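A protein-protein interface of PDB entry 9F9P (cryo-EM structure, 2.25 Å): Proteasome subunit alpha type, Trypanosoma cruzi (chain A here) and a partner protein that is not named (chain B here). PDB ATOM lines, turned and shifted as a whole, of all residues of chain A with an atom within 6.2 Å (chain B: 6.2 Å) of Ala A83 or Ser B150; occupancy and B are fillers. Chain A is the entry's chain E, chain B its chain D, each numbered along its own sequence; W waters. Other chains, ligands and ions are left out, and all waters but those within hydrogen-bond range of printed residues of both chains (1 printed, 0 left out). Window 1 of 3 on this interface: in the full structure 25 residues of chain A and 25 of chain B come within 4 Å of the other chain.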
ATOM      1  N   MET A  81      -1.320   8.105 -28.936  1.00  0.00           N
ATOM      2  CA  MET A  81      -0.036   7.516 -28.580  1.00  0.00           C
ATOM      3  C   MET A  81      -0.180   6.145 -27.919  1.00  0.00           C
ATOM      4  O   MET A  81      -0.559   6.031 -26.749  1.00  0.00           O
ATOM      5  CB  MET A  81       0.677   8.443 -27.594  1.00  0.00           C
ATOM      6  CG  MET A  81       1.097   9.760 -28.234  1.00  0.00           C
ATOM      7  SD  MET A  81       1.776  10.939 -27.024  1.00  0.00           S
ATOM      8  CE  MET A  81       2.430  12.090 -28.232  1.00  0.00           C
ATOM      9  N   VAL A  82       0.306   5.129 -28.612  1.00  0.00           N
ATOM     10  CA  VAL A  82       0.068   3.775 -28.182  1.00  0.00           C
ATOM     11  C   VAL A  82       0.672   3.455 -26.825  1.00  0.00           C
ATOM     12  O   VAL A  82       0.014   2.844 -26.001  1.00  0.00           O
ATOM     13  CB  VAL A  82       0.482   2.742 -29.252  1.00  0.00           C
ATOM     14  CG1 VAL A  82       0.515   1.326 -28.668  1.00  0.00           C
ATOM     15  CG2 VAL A  82      -0.501   2.786 -30.417  1.00  0.00           C
ATOM     16  N   ALA A  83       1.924   3.790 -26.584  1.00  0.00           N
ATOM     17  CA  ALA A  83       2.524   3.497 -25.286  1.00  0.00           C
ATOM     18  C   ALA A  83       1.819   4.181 -24.117  1.00  0.00           C
ATOM     19  O   ALA A  83       1.762   3.600 -23.041  1.00  0.00           O
ATOM     20  CB  ALA A  83       3.963   3.901 -25.326  1.00  0.00           C
ATOM     21  N   ASP A  84       1.265   5.391 -24.310  1.00  0.00           N
ATOM     22  CA  ASP A  84       0.520   6.054 -23.239  1.00  0.00           C
ATOM     23  C   ASP A  84      -0.775   5.275 -22.964  1.00  0.00           C
ATOM     24  O   ASP A  84      -1.186   5.131 -21.825  1.00  0.00           O
ATOM     25  CB  ASP A  84       0.223   7.531 -23.554  1.00  0.00           C
ATOM     26  CG  ASP A  84       1.364   8.556 -23.475  1.00  0.00           C
ATOM     27  OD1 ASP A  84       2.523   8.175 -23.106  1.00  0.00           O
ATOM     28  OD2 ASP A  84       1.098   9.769 -23.807  1.00  0.00           O
ATOM     29  N   ALA A  85      -1.408   4.764 -24.014  1.00  0.00           N
ATOM     30  CA  ALA A  85      -2.656   4.026 -23.904  1.00  0.00           C
ATOM     31  C   ALA A  85      -2.526   2.760 -23.067  1.00  0.00           C
ATOM     32  O   ALA A  85      -3.470   2.410 -22.384  1.00  0.00           O
ATOM     33  CB  ALA A  85      -3.138   3.629 -25.273  1.00  0.00           C
ATOM     34  N   ARG A  86      -1.397   2.047 -23.186  1.00  0.00           N
ATOM     35  CA  ARG A  86      -1.144   0.848 -22.396  1.00  0.00           C
ATOM     36  C   ARG A  86      -1.105   1.112 -20.893  1.00  0.00           C
ATOM     37  O   ARG A  86      -1.426   0.216 -20.128  1.00  0.00           O
ATOM     38  CB  ARG A  86       0.184   0.191 -22.778  1.00  0.00           C
ATOM     39  CG  ARG A  86       0.183  -0.351 -24.192  1.00  0.00           C
ATOM     40  CD  ARG A  86       1.577  -0.790 -24.570  1.00  0.00           C
ATOM     41  NE  ARG A  86       1.680  -1.268 -25.949  1.00  0.00           N
ATOM     42  CZ  ARG A  86       2.834  -1.423 -26.608  1.00  0.00           C
ATOM     43  NH1 ARG A  86       2.837  -1.880 -27.850  1.00  0.00           N
ATOM     44  NH2 ARG A  86       3.988  -1.120 -26.026  1.00  0.00           N
ATOM     45  N   ILE A  87      -0.725   2.309 -20.451  1.00  0.00           N
ATOM     46  CA  ILE A  87      -0.775   2.616 -19.030  1.00  0.00           C
ATOM     47  C   ILE A  87      -2.229   2.685 -18.561  1.00  0.00           C
ATOM     48  O   ILE A  87      -2.547   2.189 -17.476  1.00  0.00           O
ATOM     49  CB  ILE A  87      -0.041   3.927 -18.715  1.00  0.00           C
ATOM     50  CG1 ILE A  87       1.386   3.966 -19.242  1.00  0.00           C
ATOM     51  CG2 ILE A  87      -0.015   4.202 -17.229  1.00  0.00           C
ATOM     52  CD1 ILE A  87       2.328   3.129 -18.415  1.00  0.00           C
ATOM     53  N   LEU A  88      -3.107   3.288 -19.371  1.00  0.00           N
ATOM     54  CA  LEU A  88      -4.509   3.479 -19.015  1.00  0.00           C
ATOM     55  C   LEU A  88      -5.256   2.164 -18.993  1.00  0.00           C
ATOM     56  O   LEU A  88      -6.079   1.923 -18.126  1.00  0.00           O
ATOM     57  CB  LEU A  88      -5.190   4.402 -20.033  1.00  0.00           C
ATOM     58  CG  LEU A  88      -4.775   5.868 -19.952  1.00  0.00           C
ATOM     59  CD1 LEU A  88      -5.603   6.729 -20.870  1.00  0.00           C
ATOM     60  CD2 LEU A  88      -4.903   6.389 -18.538  1.00  0.00           C
ATOM     61  N   VAL A 139      -4.130  10.490 -25.563  1.00  0.00           N
ATOM     62  CA  VAL A 139      -4.885   9.272 -25.797  1.00  0.00           C
ATOM     63  C   VAL A 139      -6.368   9.579 -25.684  1.00  0.00           C
ATOM     64  O   VAL A 139      -6.761  10.280 -24.774  1.00  0.00           O
ATOM     65  CB  VAL A 139      -4.502   8.264 -24.704  1.00  0.00           C
ATOM     66  CG1 VAL A 139      -5.325   6.989 -24.765  1.00  0.00           C
ATOM     67  CG2 VAL A 139      -3.024   7.946 -24.764  1.00  0.00           C
ATOM     68  N   VAL B  19      10.975  13.828 -27.106  1.00  0.00           N
ATOM     69  CA  VAL B  19      10.934  12.474 -27.628  1.00  0.00           C
ATOM     70  C   VAL B  19      11.462  12.436 -29.049  1.00  0.00           C
ATOM     71  O   VAL B  19      12.167  11.492 -29.343  1.00  0.00           O
ATOM     72  CB  VAL B  19       9.583  11.755 -27.504  1.00  0.00           C
ATOM     73  CG1 VAL B  19       9.598  10.395 -28.192  1.00  0.00           C
ATOM     74  CG2 VAL B  19       9.205  11.565 -26.037  1.00  0.00           C
ATOM     75  N   GLN B  23      14.822  10.498 -30.646  1.00  0.00           N
ATOM     76  CA  GLN B  23      14.779   9.679 -31.845  1.00  0.00           C
ATOM     77  C   GLN B  23      15.866  10.125 -32.838  1.00  0.00           C
ATOM     78  O   GLN B  23      16.386   9.298 -33.544  1.00  0.00           O
ATOM     79  CB  GLN B  23      13.326   9.619 -32.327  1.00  0.00           C
ATOM     80  CG  GLN B  23      13.078   8.720 -33.531  1.00  0.00           C
ATOM     81  CD  GLN B  23      13.442   7.250 -33.375  1.00  0.00           C
ATOM     82  OE1 GLN B  23      12.890   6.514 -32.555  1.00  0.00           O
ATOM     83  NE2 GLN B  23      14.360   6.788 -34.213  1.00  0.00           N
ATOM     84  N   ALA B 112       9.870  -1.724 -22.577  1.00  0.00           N
ATOM     85  CA  ALA B 112       9.063  -0.649 -23.140  1.00  0.00           C
ATOM     86  C   ALA B 112       8.385   0.247 -22.086  1.00  0.00           C
ATOM     87  O   ALA B 112       8.297   1.456 -22.229  1.00  0.00           O
ATOM     88  CB  ALA B 112       8.042  -1.265 -24.058  1.00  0.00           C
ATOM     89  N   GLN B 115      10.991   2.706 -20.706  1.00  0.00           N
ATOM     90  CA  GLN B 115      11.157   3.804 -21.651  1.00  0.00           C
ATOM     91  C   GLN B 115       9.982   4.792 -21.629  1.00  0.00           C
ATOM     92  O   GLN B 115      10.216   5.994 -21.655  1.00  0.00           O
ATOM     93  CB  GLN B 115      11.416   3.266 -23.068  1.00  0.00           C
ATOM     94  CG  GLN B 115      12.727   2.488 -23.132  1.00  0.00           C
ATOM     95  CD  GLN B 115      13.292   2.256 -24.515  1.00  0.00           C
ATOM     96  OE1 GLN B 115      13.231   1.164 -25.076  1.00  0.00           O
ATOM     97  NE2 GLN B 115      13.976   3.278 -25.009  1.00  0.00           N
ATOM     98  N   GLN B 116       8.739   4.313 -21.666  1.00  0.00           N
ATOM     99  CA  GLN B 116       7.571   5.182 -21.657  1.00  0.00           C
ATOM    100  C   GLN B 116       7.545   6.069 -20.416  1.00  0.00           C
ATOM    101  O   GLN B 116       7.287   7.250 -20.531  1.00  0.00           O
ATOM    102  CB  GLN B 116       6.284   4.355 -21.698  1.00  0.00           C
ATOM    103  CG  GLN B 116       5.002   5.143 -21.921  1.00  0.00           C
ATOM    104  CD  GLN B 116       4.475   5.881 -20.716  1.00  0.00           C
ATOM    105  OE1 GLN B 116       4.533   5.443 -19.565  1.00  0.00           O
ATOM    106  NE2 GLN B 116       3.946   7.054 -20.980  1.00  0.00           N
ATOM    107  N   LYS B 117       7.873   5.523 -19.252  1.00  0.00           N
ATOM    108  CA  LYS B 117       7.853   6.306 -18.033  1.00  0.00           C
ATOM    109  C   LYS B 117       8.850   7.453 -18.054  1.00  0.00           C
ATOM    110  O   LYS B 117       8.617   8.448 -17.386  1.00  0.00           O
ATOM    111  CB  LYS B 117       8.139   5.469 -16.786  1.00  0.00           C
ATOM    112  CG  LYS B 117       6.923   4.697 -16.310  1.00  0.00           C
ATOM    113  CD  LYS B 117       7.115   3.969 -15.012  1.00  0.00           C
ATOM    114  CE  LYS B 117       6.032   2.923 -14.838  1.00  0.00           C
ATOM    115  NZ  LYS B 117       6.211   2.147 -13.585  1.00  0.00           N
ATOM    116  N   THR B 119       9.408   9.289 -20.403  1.00  0.00           N
ATOM    117  CA  THR B 119       8.884  10.392 -21.202  1.00  0.00           C
ATOM    118  C   THR B 119       7.799  11.176 -20.473  1.00  0.00           C
ATOM    119  O   THR B 119       7.220  12.064 -21.078  1.00  0.00           O
ATOM    120  CB  THR B 119       8.240   9.940 -22.525  1.00  0.00           C
ATOM    121  OG1 THR B 119       7.059   9.181 -22.271  1.00  0.00           O
ATOM    122  CG2 THR B 119       9.190   9.113 -23.362  1.00  0.00           C
ATOM    123  N   ASP B 148      11.204   1.571 -29.368  1.00  0.00           N
ATOM    124  CA  ASP B 148      11.733   2.923 -29.614  1.00  0.00           C
ATOM    125  C   ASP B 148      11.756   3.764 -28.327  1.00  0.00           C
ATOM    126  O   ASP B 148      11.246   3.356 -27.303  1.00  0.00           O
ATOM    127  CB  ASP B 148      11.042   3.576 -30.806  1.00  0.00           C
ATOM    128  CG  ASP B 148       9.657   4.086 -30.464  1.00  0.00           C
ATOM    129  OD1 ASP B 148       8.793   3.232 -30.217  1.00  0.00           O
ATOM    130  OD2 ASP B 148       9.454   5.350 -30.412  1.00  0.00           O
ATOM    131  N   PRO B 149      12.326   4.987 -28.333  1.00  0.00           N
ATOM    132  CA  PRO B 149      12.353   5.858 -27.148  1.00  0.00           C
ATOM    133  C   PRO B 149      11.034   6.334 -26.547  1.00  0.00           C
ATOM    134  O   PRO B 149      11.024   6.659 -25.375  1.00  0.00           O
ATOM    135  CB  PRO B 149      13.076   7.115 -27.634  1.00  0.00           C
ATOM    136  CG  PRO B 149      13.892   6.642 -28.805  1.00  0.00           C
ATOM    137  CD  PRO B 149      12.985   5.622 -29.479  1.00  0.00           C
ATOM    138  N   SER B 150       9.938   6.347 -27.318  1.00  0.00           N
ATOM    139  CA  SER B 150       8.596   6.612 -26.801  1.00  0.00           C
ATOM    140  C   SER B 150       7.985   5.463 -25.977  1.00  0.00           C
ATOM    141  O   SER B 150       6.934   5.657 -25.355  1.00  0.00           O
ATOM    142  CB  SER B 150       7.669   6.834 -27.944  1.00  0.00           C
ATOM    143  OG  SER B 150       7.445   5.599 -28.604  1.00  0.00           O
ATOM    144  N   GLY B 151       8.563   4.244 -26.053  1.00  0.00           N
ATOM    145  CA  GLY B 151       7.962   3.066 -25.451  1.00  0.00           C
ATOM    146  C   GLY B 151       7.112   2.212 -26.394  1.00  0.00           C
ATOM    147  O   GLY B 151       6.559   1.223 -25.967  1.00  0.00           O
ATOM    148  N   MET B 152       7.037   2.521 -27.672  1.00  0.00           N
ATOM    149  CA  MET B 152       6.297   1.694 -28.613  1.00  0.00           C
ATOM    150  C   MET B 152       7.072   0.404 -28.961  1.00  0.00           C
ATOM    151  O   MET B 152       8.235   0.464 -29.295  1.00  0.00           O
ATOM    152  CB  MET B 152       6.023   2.541 -29.868  1.00  0.00           C
ATOM    153  CG  MET B 152       5.094   1.900 -30.885  1.00  0.00           C
ATOM    154  SD  MET B 152       3.699   0.993 -30.102  1.00  0.00           S
ATOM    155  CE  MET B 152       3.233  -0.115 -31.436  1.00  0.00           C
HETATM  156  O   HOH W   1       5.670   8.044 -24.509  1.00  0.00           O
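The side-chain hydroxyl (OG1) of Thr B119 lies within hydrogen-bond range of the backbone carbonyl oxygen (O) of Gln B116, at 2.6 Å. The side-chain carboxylate (OD2) of Asp B148 lies within hydrogen-bond range of the side-chain hydroxyl (OG) of Ser B150. OD1 of Asp B148 lies close to N of Met B152, 3.2 Å away. OG of Ser B150 is in hydrogen-bond range of N of Met B152 (3.2 Å).
Water W1 lies within hydrogen-bond range of O of Ser B150 (2.8 Å), OG1 of Thr B119 (2.9 Å) and OD1 of Asp A84 (3.4 Å).
Of the printed residues of chain B, Val A82 touches Met B152. Ala A83 touches just these residues of chain B: Gln B116, Ser B150 and Gly B151. Printed residues of chain B within 4 Å of Asp A84: Gln B116. Printed residues of chain A within 4 Å of Gln B116: Ala A83, Asp A84 and Ile A87. Thr B119 touches none of the printed residues of chain A. Printed residues of chain A within 4 Å of Ser B150: Ala A83 (3.5 Å). The nearest residue of chain A that does not touch Ser B150 is Asp A84 (5.6 Å). The nearest printed residue of chain A that does not touch Met B152 is Ala A83 (4.1 Å).
Among the printed residues, pairs that only touch across the chains: Ile A87 with Gln B116 (3.4 Å), Ala A83 with Ser B150 (3.5 Å), Val A82 with Met B152 (3.5 Å), Ala A83 with Gly B151 (3.7 Å) and Ala A83 with Gln B116 (3.8 Å).
NE2 of Gln B116 lies within hydrogen-bond range of OD1 of Asp A84 (2.8 Å). O of Gly B151 sits at hydrogen-bond distance from NH2 of Arg A86 (3.5 Å). SD of Met B152 sits at hydrogen-bond distance from NH1 of Arg A86 (3.8 Å).
Of the 12 printed residues of chain B, 4 touch a printed residue of chain A. Printed residues of chain B that touch a printed residue of chain A: Gln B116, Ser B150, Gly B151 and Met B152. Hydrophobic or aromatic side chains of chain B that line the printed part of chain A: Met B152. Hydrophobic or aromatic side chains of chain A within 4 Å of the printed part of chain B: Val A82, Ala A83 and Ile A87. Among the printed residues, 8 pairs touch across the chains. Among the printed residues, no Asp or Glu carboxylate lies within 4 Å of a Lys or Arg side-chain nitrogen of the other chain.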
